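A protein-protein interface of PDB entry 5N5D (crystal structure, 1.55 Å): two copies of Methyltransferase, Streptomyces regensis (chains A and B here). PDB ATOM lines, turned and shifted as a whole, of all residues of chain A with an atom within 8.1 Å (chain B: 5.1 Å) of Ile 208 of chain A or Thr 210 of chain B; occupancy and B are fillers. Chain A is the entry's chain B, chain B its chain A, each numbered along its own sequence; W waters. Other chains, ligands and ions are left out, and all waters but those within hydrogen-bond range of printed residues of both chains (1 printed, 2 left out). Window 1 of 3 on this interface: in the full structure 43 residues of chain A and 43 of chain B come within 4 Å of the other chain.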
ATOM      1  N   TRP A  10      18.658 -20.446  11.524  1.00  0.00           N
ATOM      2  CA  TRP A  10      19.306 -19.158  11.737  1.00  0.00           C
ATOM      3  C   TRP A  10      19.595 -18.465  10.414  1.00  0.00           C
ATOM      4  O   TRP A  10      19.348 -17.263  10.270  1.00  0.00           O
ATOM      5  CB  TRP A  10      20.592 -19.358  12.532  1.00  0.00           C
ATOM      6  CG  TRP A  10      20.380 -19.884  13.909  1.00  0.00           C
ATOM      7  CD1 TRP A  10      19.204 -19.954  14.596  1.00  0.00           C
ATOM      8  CD2 TRP A  10      21.385 -20.403  14.777  1.00  0.00           C
ATOM      9  NE1 TRP A  10      19.417 -20.487  15.841  1.00  0.00           N
ATOM     10  CE2 TRP A  10      20.750 -20.772  15.977  1.00  0.00           C
ATOM     11  CE3 TRP A  10      22.764 -20.594  14.655  1.00  0.00           C
ATOM     12  CZ2 TRP A  10      21.445 -21.318  17.047  1.00  0.00           C
ATOM     13  CZ3 TRP A  10      23.453 -21.138  15.718  1.00  0.00           C
ATOM     14  CH2 TRP A  10      22.795 -21.495  16.897  1.00  0.00           C
ATOM     15  N   ASP A  14      17.685 -14.919   9.009  1.00  0.00           N
ATOM     16  CA  ASP A  14      18.497 -13.775   8.588  1.00  0.00           C
ATOM     17  C   ASP A  14      18.215 -13.398   7.139  1.00  0.00           C
ATOM     18  O   ASP A  14      18.105 -12.211   6.804  1.00  0.00           O
ATOM     19  CB  ASP A  14      19.986 -14.095   8.752  1.00  0.00           C
ATOM     20  CG  ASP A  14      20.650 -13.323   9.886  1.00  0.00           C
ATOM     21  OD1 ASP A  14      19.951 -12.681  10.699  1.00  0.00           O
ATOM     22  OD2 ASP A  14      21.898 -13.374   9.961  1.00  0.00           O
ATOM     23  N   PHE A  17      14.709 -11.588   7.232  1.00  0.00           N
ATOM     24  CA  PHE A  17      14.738 -10.221   7.743  1.00  0.00           C
ATOM     25  C   PHE A  17      15.491  -9.298   6.796  1.00  0.00           C
ATOM     26  O   PHE A  17      15.030  -8.191   6.480  1.00  0.00           O
ATOM     27  CB  PHE A  17      15.402 -10.178   9.120  1.00  0.00           C
ATOM     28  CG  PHE A  17      14.585 -10.765  10.235  1.00  0.00           C
ATOM     29  CD1 PHE A  17      13.212 -10.638  10.270  1.00  0.00           C
ATOM     30  CD2 PHE A  17      15.219 -11.411  11.286  1.00  0.00           C
ATOM     31  CE1 PHE A  17      12.480 -11.173  11.319  1.00  0.00           C
ATOM     32  CE2 PHE A  17      14.493 -11.941  12.328  1.00  0.00           C
ATOM     33  CZ  PHE A  17      13.127 -11.824  12.344  1.00  0.00           C
ATOM     34  N   LEU A  52      22.946  -2.643  11.682  1.00  0.00           N
ATOM     35  CA  LEU A  52      22.893  -2.248  13.086  1.00  0.00           C
ATOM     36  C   LEU A  52      23.971  -1.217  13.405  1.00  0.00           C
ATOM     37  O   LEU A  52      23.705  -0.220  14.087  1.00  0.00           O
ATOM     38  CB  LEU A  52      23.032  -3.470  13.993  1.00  0.00           C
ATOM     39  CG  LEU A  52      22.973  -3.162  15.499  1.00  0.00           C
ATOM     40  CD1 LEU A  52      21.693  -2.430  15.877  1.00  0.00           C
ATOM     41  CD2 LEU A  52      23.100  -4.429  16.323  1.00  0.00           C
ATOM     42  N   VAL A 168      32.444  -3.733  20.114  1.00  0.00           N
ATOM     43  CA  VAL A 168      33.495  -4.721  19.886  1.00  0.00           C
ATOM     44  C   VAL A 168      32.833  -5.973  19.330  1.00  0.00           C
ATOM     45  O   VAL A 168      31.941  -6.543  19.972  1.00  0.00           O
ATOM     46  CB  VAL A 168      34.267  -5.045  21.175  1.00  0.00           C
ATOM     47  CG1 VAL A 168      35.405  -6.014  20.885  1.00  0.00           C
ATOM     48  CG2 VAL A 168      34.791  -3.757  21.826  1.00  0.00           C
ATOM     49  N   ASP A 169      33.276  -6.412  18.157  1.00  0.00           N
ATOM     50  CA  ASP A 169      32.690  -7.583  17.522  1.00  0.00           C
ATOM     51  C   ASP A 169      33.398  -8.863  17.967  1.00  0.00           C
ATOM     52  O   ASP A 169      34.543  -8.850  18.425  1.00  0.00           O
ATOM     53  CB  ASP A 169      32.746  -7.463  15.995  1.00  0.00           C
ATOM     54  CG  ASP A 169      31.685  -8.302  15.299  1.00  0.00           C
ATOM     55  OD1 ASP A 169      30.790  -8.851  15.978  1.00  0.00           O
ATOM     56  OD2 ASP A 169      31.745  -8.405  14.058  1.00  0.00           O
ATOM     57  N   ASN A 170      32.675  -9.977  17.835  1.00  0.00           N
ATOM     58  CA  ASN A 170      33.227 -11.332  17.921  1.00  0.00           C
ATOM     59  C   ASN A 170      33.766 -11.656  19.314  1.00  0.00           C
ATOM     60  O   ASN A 170      34.857 -12.206  19.455  1.00  0.00           O
ATOM     61  CB  ASN A 170      34.318 -11.548  16.867  1.00  0.00           C
ATOM     62  CG  ASN A 170      33.840 -11.275  15.465  1.00  0.00           C
ATOM     63  OD1 ASN A 170      34.425 -10.464  14.745  1.00  0.00           O
ATOM     64  ND2 ASN A 170      32.780 -11.960  15.058  1.00  0.00           N
ATOM     65  N   VAL A 171      32.961 -11.384  20.344  1.00  0.00           N
ATOM     66  CA  VAL A 171      33.413 -11.542  21.724  1.00  0.00           C
ATOM     67  C   VAL A 171      33.026 -12.884  22.333  1.00  0.00           C
ATOM     68  O   VAL A 171      33.378 -13.141  23.490  1.00  0.00           O
ATOM     69  CB  VAL A 171      32.897 -10.407  22.635  1.00  0.00           C
ATOM     70  CG1 VAL A 171      33.443  -9.073  22.172  1.00  0.00           C
ATOM     71  CG2 VAL A 171      31.359 -10.385  22.701  1.00  0.00           C
ATOM     72  N   VAL A 172      32.324 -13.749  21.607  1.00  0.00           N
ATOM     73  CA  VAL A 172      31.826 -14.982  22.224  1.00  0.00           C
ATOM     74  C   VAL A 172      32.795 -16.146  22.038  1.00  0.00           C
ATOM     75  O   VAL A 172      32.954 -16.972  22.942  1.00  0.00           O
ATOM     76  CB  VAL A 172      30.425 -15.300  21.665  1.00  0.00           C
ATOM     77  CG1 VAL A 172      30.007 -16.728  21.972  1.00  0.00           C
ATOM     78  CG2 VAL A 172      29.422 -14.325  22.259  1.00  0.00           C
ATOM     79  N   HIS A 194      36.577  -7.634  29.226  1.00  0.00           N
ATOM     80  CA  HIS A 194      35.373  -7.624  30.049  1.00  0.00           C
ATOM     81  C   HIS A 194      35.709  -7.358  31.509  1.00  0.00           C
ATOM     82  O   HIS A 194      34.961  -6.666  32.207  1.00  0.00           O
ATOM     83  CB  HIS A 194      34.609  -8.932  29.871  1.00  0.00           C
ATOM     84  CG  HIS A 194      33.849  -8.982  28.586  1.00  0.00           C
ATOM     85  ND1 HIS A 194      34.457  -9.223  27.375  1.00  0.00           N
ATOM     86  CD2 HIS A 194      32.539  -8.764  28.317  1.00  0.00           C
ATOM     87  CE1 HIS A 194      33.551  -9.166  26.413  1.00  0.00           C
ATOM     88  NE2 HIS A 194      32.379  -8.898  26.960  1.00  0.00           N
ATOM     89  N   ALA A 205      28.391  -1.002  29.942  1.00  0.00           N
ATOM     90  CA  ALA A 205      28.326  -1.838  28.754  1.00  0.00           C
ATOM     91  C   ALA A 205      27.394  -3.030  28.944  1.00  0.00           C
ATOM     92  O   ALA A 205      26.928  -3.333  30.048  1.00  0.00           O
ATOM     93  CB  ALA A 205      29.726  -2.327  28.369  1.00  0.00           C
ATOM     94  N   THR A 206      27.118  -3.690  27.823  1.00  0.00           N
ATOM     95  CA  THR A 206      26.409  -4.959  27.802  1.00  0.00           C
ATOM     96  C   THR A 206      26.962  -5.793  26.656  1.00  0.00           C
ATOM     97  O   THR A 206      27.576  -5.274  25.724  1.00  0.00           O
ATOM     98  CB  THR A 206      24.890  -4.767  27.657  1.00  0.00           C
ATOM     99  OG1 THR A 206      24.222  -5.998  27.949  1.00  0.00           O
ATOM    100  CG2 THR A 206      24.517  -4.306  26.246  1.00  0.00           C
ATOM    101  N   SER A 207      26.758  -7.099  26.743  1.00  0.00           N
ATOM    102  CA  SER A 207      27.205  -8.019  25.707  1.00  0.00           C
ATOM    103  C   SER A 207      26.035  -8.898  25.304  1.00  0.00           C
ATOM    104  O   SER A 207      25.287  -9.390  26.156  1.00  0.00           O
ATOM    105  CB  SER A 207      28.395  -8.884  26.163  1.00  0.00           C
ATOM    106  OG  SER A 207      29.593  -8.122  26.219  1.00  0.00           O
ATOM    107  N   ILE A 208      25.876  -9.070  23.996  1.00  0.00           N
ATOM    108  CA  ILE A 208      24.724  -9.732  23.399  1.00  0.00           C
ATOM    109  C   ILE A 208      25.224 -10.888  22.547  1.00  0.00           C
ATOM    110  O   ILE A 208      26.095 -10.692  21.692  1.00  0.00           O
ATOM    111  CB  ILE A 208      23.913  -8.741  22.544  1.00  0.00           C
ATOM    112  CG1 ILE A 208      23.415  -7.570  23.400  1.00  0.00           C
ATOM    113  CG2 ILE A 208      22.765  -9.446  21.819  1.00  0.00           C
ATOM    114  CD1 ILE A 208      22.382  -7.939  24.435  1.00  0.00           C
ATOM    115  N   GLN A 209      24.681 -12.088  22.779  1.00  0.00           N
ATOM    116  CA  GLN A 209      24.961 -13.248  21.939  1.00  0.00           C
ATOM    117  C   GLN A 209      24.005 -13.239  20.750  1.00  0.00           C
ATOM    118  O   GLN A 209      22.790 -13.119  20.931  1.00  0.00           O
ATOM    119  CB  GLN A 209      24.797 -14.561  22.722  1.00  0.00           C
ATOM    120  CG  GLN A 209      25.483 -14.640  24.121  1.00  0.00           C
ATOM    121  CD  GLN A 209      25.111 -15.908  24.939  1.00  0.00           C
ATOM    122  OE1 GLN A 209      25.334 -17.043  24.515  1.00  0.00           O
ATOM    123  NE2 GLN A 209      24.549 -15.696  26.124  1.00  0.00           N
ATOM    124  N   THR A 210      24.550 -13.375  19.548  1.00  0.00           N
ATOM    125  CA  THR A 210      23.755 -13.357  18.334  1.00  0.00           C
ATOM    126  C   THR A 210      23.930 -14.661  17.570  1.00  0.00           C
ATOM    127  O   THR A 210      24.923 -15.378  17.725  1.00  0.00           O
ATOM    128  CB  THR A 210      24.141 -12.193  17.420  1.00  0.00           C
ATOM    129  OG1 THR A 210      25.487 -12.376  16.959  1.00  0.00           O
ATOM    130  CG2 THR A 210      24.018 -10.857  18.150  1.00  0.00           C
ATOM    131  N   VAL A 211      22.936 -14.955  16.736  1.00  0.00           N
ATOM    132  CA  VAL A 211      23.017 -16.020  15.753  1.00  0.00           C
ATOM    133  C   VAL A 211      22.498 -15.473  14.430  1.00  0.00           C
ATOM    134  O   VAL A 211      21.896 -14.398  14.361  1.00  0.00           O
ATOM    135  CB  VAL A 211      22.239 -17.287  16.176  1.00  0.00           C
ATOM    136  CG1 VAL A 211      22.787 -17.839  17.487  1.00  0.00           C
ATOM    137  CG2 VAL A 211      20.740 -17.008  16.293  1.00  0.00           C
ATOM    138  N   GLY A 212      22.756 -16.223  13.373  1.00  0.00           N
ATOM    139  CA  GLY A 212      22.414 -15.803  12.027  1.00  0.00           C
ATOM    140  C   GLY A 212      23.287 -16.532  11.018  1.00  0.00           C
ATOM    141  O   GLY A 212      23.776 -17.626  11.283  1.00  0.00           O
ATOM    142  N   TYR A 216      26.904 -18.731  15.669  1.00  0.00           N
ATOM    143  CA  TYR A 216      26.824 -18.246  17.039  1.00  0.00           C
ATOM    144  C   TYR A 216      28.036 -17.380  17.359  1.00  0.00           C
ATOM    145  O   TYR A 216      29.180 -17.807  17.176  1.00  0.00           O
ATOM    146  CB  TYR A 216      26.748 -19.451  17.976  1.00  0.00           C
ATOM    147  CG  TYR A 216      26.866 -19.182  19.458  1.00  0.00           C
ATOM    148  CD1 TYR A 216      25.958 -18.376  20.124  1.00  0.00           C
ATOM    149  CD2 TYR A 216      27.859 -19.798  20.202  1.00  0.00           C
ATOM    150  CE1 TYR A 216      26.064 -18.161  21.495  1.00  0.00           C
ATOM    151  CE2 TYR A 216      27.970 -19.597  21.554  1.00  0.00           C
ATOM    152  CZ  TYR A 216      27.071 -18.785  22.200  1.00  0.00           C
ATOM    153  OH  TYR A 216      27.198 -18.595  23.560  1.00  0.00           O
ATOM    154  N   ASP A 217      27.782 -16.162  17.823  1.00  0.00           N
ATOM    155  CA  ASP A 217      28.833 -15.213  18.177  1.00  0.00           C
ATOM    156  C   ASP A 217      28.189 -14.126  19.039  1.00  0.00           C
ATOM    157  O   ASP A 217      27.144 -14.354  19.657  1.00  0.00           O
ATOM    158  CB  ASP A 217      29.513 -14.664  16.912  1.00  0.00           C
ATOM    159  CG  ASP A 217      30.976 -14.324  17.138  1.00  0.00           C
ATOM    160  OD1 ASP A 217      31.362 -14.071  18.298  1.00  0.00           O
ATOM    161  OD2 ASP A 217      31.737 -14.323  16.148  1.00  0.00           O
ATOM    162  N   GLY A 218      28.793 -12.947  19.079  1.00  0.00           N
ATOM    163  CA  GLY A 218      28.230 -11.883  19.886  1.00  0.00           C
ATOM    164  C   GLY A 218      29.087 -10.641  19.821  1.00  0.00           C
ATOM    165  O   GLY A 218      30.186 -10.641  19.258  1.00  0.00           O
ATOM    166  N   PHE A 219      28.553  -9.573  20.409  1.00  0.00           N
ATOM    167  CA  PHE A 219      29.211  -8.276  20.421  1.00  0.00           C
ATOM    168  C   PHE A 219      29.019  -7.629  21.782  1.00  0.00           C
ATOM    169  O   PHE A 219      28.091  -7.951  22.526  1.00  0.00           O
ATOM    170  CB  PHE A 219      28.664  -7.351  19.326  1.00  0.00           C
ATOM    171  CG  PHE A 219      27.237  -6.923  19.538  1.00  0.00           C
ATOM    172  CD1 PHE A 219      26.186  -7.717  19.107  1.00  0.00           C
ATOM    173  CD2 PHE A 219      26.943  -5.721  20.156  1.00  0.00           C
ATOM    174  CE1 PHE A 219      24.868  -7.312  19.293  1.00  0.00           C
ATOM    175  CE2 PHE A 219      25.628  -5.318  20.345  1.00  0.00           C
ATOM    176  CZ  PHE A 219      24.596  -6.108  19.913  1.00  0.00           C
ATOM    177  N   THR A 220      29.902  -6.679  22.083  1.00  0.00           N
ATOM    178  CA  THR A 220      29.800  -5.834  23.262  1.00  0.00           C
ATOM    179  C   THR A 220      29.515  -4.408  22.822  1.00  0.00           C
ATOM    180  O   THR A 220      30.114  -3.918  21.862  1.00  0.00           O
ATOM    181  CB  THR A 220      31.089  -5.879  24.086  1.00  0.00           C
ATOM    182  OG1 THR A 220      31.326  -7.220  24.497  1.00  0.00           O
ATOM    183  CG2 THR A 220      30.994  -4.983  25.324  1.00  0.00           C
ATOM    184  N   LEU A 221      28.599  -3.751  23.527  1.00  0.00           N
ATOM    185  CA  LEU A 221      28.268  -2.357  23.284  1.00  0.00           C
ATOM    186  C   LEU A 221      28.502  -1.596  24.578  1.00  0.00           C
ATOM    187  O   LEU A 221      27.947  -1.956  25.623  1.00  0.00           O
ATOM    188  CB  LEU A 221      26.826  -2.206  22.792  1.00  0.00           C
ATOM    189  CG  LEU A 221      26.429  -0.779  22.408  1.00  0.00           C
ATOM    190  CD1 LEU A 221      25.350  -0.825  21.334  1.00  0.00           C
ATOM    191  CD2 LEU A 221      25.937   0.017  23.606  1.00  0.00           C
ATOM    192  N   PRO B  48      21.198  -8.590  30.306  1.00  0.00           N
ATOM    193  CA  PRO B  48      21.937  -7.948  29.204  1.00  0.00           C
ATOM    194  C   PRO B  48      21.028  -7.217  28.232  1.00  0.00           C
ATOM    195  O   PRO B  48      21.404  -6.160  27.705  1.00  0.00           O
ATOM    196  CB  PRO B  48      22.660  -9.125  28.532  1.00  0.00           C
ATOM    197  CG  PRO B  48      22.720 -10.200  29.576  1.00  0.00           C
ATOM    198  CD  PRO B  48      21.454 -10.040  30.362  1.00  0.00           C
ATOM    199  N   GLN B  49      19.827  -7.754  27.992  1.00  0.00           N
ATOM    200  CA  GLN B  49      18.868  -7.120  27.087  1.00  0.00           C
ATOM    201  C   GLN B  49      18.289  -5.840  27.677  1.00  0.00           C
ATOM    202  O   GLN B  49      18.116  -4.841  26.963  1.00  0.00           O
ATOM    203  CB  GLN B  49      17.731  -8.092  26.777  1.00  0.00           C
ATOM    204  CG  GLN B  49      18.102  -9.259  25.903  1.00  0.00           C
ATOM    205  CD  GLN B  49      16.989 -10.304  25.828  1.00  0.00           C
ATOM    206  OE1 GLN B  49      15.997 -10.236  26.565  1.00  0.00           O
ATOM    207  NE2 GLN B  49      17.156 -11.274  24.946  1.00  0.00           N
ATOM    208  N   LEU B  52      20.865  -3.288  27.373  1.00  0.00           N
ATOM    209  CA  LEU B  52      20.939  -2.764  26.015  1.00  0.00           C
ATOM    210  C   LEU B  52      19.847  -1.725  25.765  1.00  0.00           C
ATOM    211  O   LEU B  52      20.112  -0.673  25.175  1.00  0.00           O
ATOM    212  CB  LEU B  52      20.841  -3.898  24.995  1.00  0.00           C
ATOM    213  CG  LEU B  52      20.907  -3.424  23.537  1.00  0.00           C
ATOM    214  CD1 LEU B  52      22.177  -2.601  23.258  1.00  0.00           C
ATOM    215  CD2 LEU B  52      20.822  -4.612  22.602  1.00  0.00           C
ATOM    216  N   ILE B 208      17.792  -8.544  14.577  1.00  0.00           N
ATOM    217  CA  ILE B 208      18.938  -9.271  15.104  1.00  0.00           C
ATOM    218  C   ILE B 208      18.421 -10.480  15.864  1.00  0.00           C
ATOM    219  O   ILE B 208      17.604 -10.334  16.783  1.00  0.00           O
ATOM    220  CB  ILE B 208      19.790  -8.381  16.021  1.00  0.00           C
ATOM    221  CG1 ILE B 208      20.316  -7.160  15.264  1.00  0.00           C
ATOM    222  CG2 ILE B 208      20.950  -9.173  16.618  1.00  0.00           C
ATOM    223  CD1 ILE B 208      21.268  -7.481  14.129  1.00  0.00           C
ATOM    224  N   GLN B 209      18.896 -11.666  15.487  1.00  0.00           N
ATOM    225  CA  GLN B 209      18.599 -12.883  16.232  1.00  0.00           C
ATOM    226  C   GLN B 209      19.576 -13.032  17.393  1.00  0.00           C
ATOM    227  O   GLN B 209      20.783 -12.820  17.237  1.00  0.00           O
ATOM    228  CB  GLN B 209      18.698 -14.109  15.326  1.00  0.00           C
ATOM    229  CG  GLN B 209      17.871 -14.081  14.048  1.00  0.00           C
ATOM    230  CD  GLN B 209      18.149 -15.309  13.162  1.00  0.00           C
ATOM    231  OE1 GLN B 209      17.800 -16.435  13.511  1.00  0.00           O
ATOM    232  NE2 GLN B 209      18.796 -15.086  12.025  1.00  0.00           N
ATOM    233  N   THR B 210      19.052 -13.412  18.559  1.00  0.00           N
ATOM    234  CA  THR B 210      19.857 -13.528  19.767  1.00  0.00           C
ATOM    235  C   THR B 210      19.608 -14.865  20.456  1.00  0.00           C
ATOM    236  O   THR B 210      18.586 -15.519  20.251  1.00  0.00           O
ATOM    237  CB  THR B 210      19.558 -12.393  20.764  1.00  0.00           C
ATOM    238  OG1 THR B 210      18.205 -12.494  21.216  1.00  0.00           O
ATOM    239  CG2 THR B 210      19.768 -11.029  20.123  1.00  0.00           C
ATOM    240  N   VAL B 211      20.571 -15.259  21.288  1.00  0.00           N
ATOM    241  CA  VAL B 211      20.407 -16.364  22.222  1.00  0.00           C
ATOM    242  C   VAL B 211      20.953 -15.905  23.567  1.00  0.00           C
ATOM    243  O   VAL B 211      21.533 -14.824  23.692  1.00  0.00           O
ATOM    244  CB  VAL B 211      21.099 -17.665  21.756  1.00  0.00           C
ATOM    245  CG1 VAL B 211      20.510 -18.142  20.429  1.00  0.00           C
ATOM    246  CG2 VAL B 211      22.618 -17.488  21.664  1.00  0.00           C
ATOM    247  N   GLY B 212      20.751 -16.736  24.576  1.00  0.00           N
ATOM    248  CA  GLY B 212      21.051 -16.378  25.944  1.00  0.00           C
ATOM    249  C   GLY B 212      20.036 -17.014  26.870  1.00  0.00           C
ATOM    250  O   GLY B 212      19.380 -17.983  26.506  1.00  0.00           O
ATOM    251  N   GLY B 215      16.654 -18.030  25.644  1.00  0.00           N
ATOM    252  CA  GLY B 215      16.579 -18.923  24.510  1.00  0.00           C
ATOM    253  C   GLY B 215      16.759 -18.163  23.208  1.00  0.00           C
ATOM    254  O   GLY B 215      17.231 -17.026  23.175  1.00  0.00           O
ATOM    255  N   TYR B 216      16.359 -18.817  22.120  1.00  0.00           N
ATOM    256  CA  TYR B 216      16.494 -18.265  20.777  1.00  0.00           C
ATOM    257  C   TYR B 216      15.327 -17.334  20.469  1.00  0.00           C
ATOM    258  O   TYR B 216      14.162 -17.746  20.541  1.00  0.00           O
ATOM    259  CB  TYR B 216      16.555 -19.415  19.772  1.00  0.00           C
ATOM    260  CG  TYR B 216      16.404 -19.051  18.313  1.00  0.00           C
ATOM    261  CD1 TYR B 216      17.250 -18.136  17.704  1.00  0.00           C
ATOM    262  CD2 TYR B 216      15.445 -19.677  17.526  1.00  0.00           C
ATOM    263  CE1 TYR B 216      17.122 -17.829  16.357  1.00  0.00           C
ATOM    264  CE2 TYR B 216      15.315 -19.380  16.186  1.00  0.00           C
ATOM    265  CZ  TYR B 216      16.154 -18.457  15.608  1.00  0.00           C
ATOM    266  OH  TYR B 216      16.025 -18.164  14.265  1.00  0.00           O
ATOM    267  N   ASP B 217      15.644 -16.084  20.130  1.00  0.00           N
ATOM    268  CA  ASP B 217      14.629 -15.117  19.727  1.00  0.00           C
ATOM    269  C   ASP B 217      15.332 -13.977  18.983  1.00  0.00           C
ATOM    270  O   ASP B 217      16.400 -14.180  18.402  1.00  0.00           O
ATOM    271  CB  ASP B 217      13.848 -14.660  20.976  1.00  0.00           C
ATOM    272  CG  ASP B 217      12.463 -14.149  20.649  1.00  0.00           C
ATOM    273  OD1 ASP B 217      12.141 -14.004  19.450  1.00  0.00           O
ATOM    274  OD2 ASP B 217      11.696 -13.896  21.601  1.00  0.00           O
ATOM    275  N   GLY B 218      14.732 -12.791  19.002  1.00  0.00           N
ATOM    276  CA  GLY B 218      15.348 -11.661  18.322  1.00  0.00           C
ATOM    277  C   GLY B 218      14.528 -10.402  18.492  1.00  0.00           C
ATOM    278  O   GLY B 218      13.404 -10.425  19.003  1.00  0.00           O
ATOM    279  N   PHE B 219      15.110  -9.291  18.038  1.00  0.00           N
ATOM    280  CA  PHE B 219      14.461  -7.996  18.129  1.00  0.00           C
ATOM    281  C   PHE B 219      14.664  -7.225  16.837  1.00  0.00           C
ATOM    282  O   PHE B 219      15.570  -7.514  16.049  1.00  0.00           O
ATOM    283  CB  PHE B 219      15.004  -7.185  19.309  1.00  0.00           C
ATOM    284  CG  PHE B 219      16.452  -6.773  19.157  1.00  0.00           C
ATOM    285  CD1 PHE B 219      17.478  -7.624  19.526  1.00  0.00           C
ATOM    286  CD2 PHE B 219      16.779  -5.518  18.673  1.00  0.00           C
ATOM    287  CE1 PHE B 219      18.811  -7.236  19.407  1.00  0.00           C
ATOM    288  CE2 PHE B 219      18.102  -5.122  18.543  1.00  0.00           C
ATOM    289  CZ  PHE B 219      19.121  -5.980  18.915  1.00  0.00           C
HETATM  290  O   HOH W   1      22.062 -12.277  24.320  1.00  0.00           O
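Water W1 bridges the backbone carbonyl oxygen (O) of Val 211 of chain B and the backbone NH (N) of Gln 209 of chain A.
The side-chain hydroxyl (OG1) of Thr 206 of chain A sits at hydrogen-bond distance from the backbone carbonyl oxygen (O) of Pro 48 of chain B.
The side-chain amide nitrogen of Gln 209 of chain B lies within hydrogen-bond range of the backbone carbonyl oxygen of Trp 10 of chain A (2.9 Å).
The side-chain amide nitrogen (NE2) of Gln 209 of chain B lies within hydrogen-bond range of the side-chain carboxylate (OD1) of Asp 14 of chain A (3.0 Å).
O of Gln 209 of chain B lies within hydrogen-bond range of N of Val 211 of chain A (3.1 Å).
N of Val 211 of chain B sits at hydrogen-bond distance from O of Gln 209 of chain A, 3.1 Å away.
Printed residues of chain B within 4 Å of Ile 208 of chain A: Pro 48 and Thr 210.
Of the printed residues of chain A, Thr 210 of chain B touches Ile 208 and Gln 209.
Of the printed residues of chain A, Val 211 of chain B touches Gln 209 (3.1 Å), Val 211 (3.7 Å) and Tyr 216 (3.5 Å).
Of the printed residues of chain B, Trp 10 of chain A touches Gln 209 (2.9 Å) and Tyr 216 (3.5 Å).
The nearest printed residue of chain B that does not touch Ile 208 of chain A is Leu 52 of chain B (4.01 Å).
The nearest printed residue of chain A that does not touch Pro 48 of chain B is Ala 205 of chain A (6.6 Å).
Among the printed residues, pairs that only touch across the chains: Gln 209 of chain A with Thr 210 of chain B, Thr 210 of chain A with Gln 209 of chain B, Trp 10 of chain A with Tyr 216 of chain B, Tyr 216 of chain A with Val 211 of chain B, Ser 207 of chain A with Pro 48 of chain B, Gln 209 of chain A with Gly 212 of chain B, Gly 212 of chain A with Gln 209 of chain B, Val 211 of chain A with Tyr 216 of chain B, Val 211 of chain A with Val 211 of chain B, Ile 208 of chain A with Thr 210 of chain B, Thr 210 of chain A with Ile 208 of chain B, Ile 208 of chain A with Pro 48 of chain B and Thr 206 of chain A with Leu 52 of chain B.
Gln 209 of chain A touches Thr 210 of chain B, and with the chains exchanged Thr 210 of chain A touches Gln 209 of chain B.
Gln 209 of chain A touches Val 211 of chain B, and with the chains exchanged Val 211 of chain A touches Gln 209 of chain B.
Val 211 of chain A touches its own counterpart, Val 211 of chain B.
Val 211 of chain A touches Tyr 216 of chain B, and with the chains exchanged Tyr 216 of chain A touches Val 211 of chain B.
10 positions are printed for both chains.
The side-chain amide oxygen of Gln 209 of chain B is in hydrogen-bond range of the side-chain hydroxyl of Tyr 216 of chain B (2.6 Å).
The backbone NH (N) of Thr 210 of chain B lies within hydrogen-bond range of the backbone carbonyl oxygen (O) of Asp 217 of chain B (2.8 Å).
A ring nitrogen (NE2) of His 194 of chain A sits at hydrogen-bond distance from the side-chain hydroxyl of Ser 207 of chain A (3.0 Å).
The backbone NH of Leu 221 of chain A lies within hydrogen-bond range of the backbone carbonyl oxygen of Thr 206 of chain A (2.9 Å).
The backbone NH of Ile 208 of chain A sits at hydrogen-bond distance from the backbone carbonyl oxygen of Phe 219 of chain A, 2.9 Å away.
The side-chain amide oxygen of Gln 209 of chain A sits at hydrogen-bond distance from the side-chain hydroxyl of Tyr 216 of chain A (2.6 Å).
Of the 13 printed residues of chain B, 8 touch a printed residue of chain A.
Hydrophobic or aromatic side chains of chain B that line the printed part of chain A: Pro 48, Leu 52, Ile 208, Val 211 and Tyr 216.
Printed residues of chain A that touch a printed residue of chain B: Trp 10, Asp 14, Thr 206, Ser 207, Ile 208, Gln 209, Thr 210, Val 211, Gly 212 and Tyr 216.
Hydrophobic or aromatic side chains of chain A within 4 Å of the printed part of chain B: Trp 10, Ile 208, Val 211 and Tyr 216.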
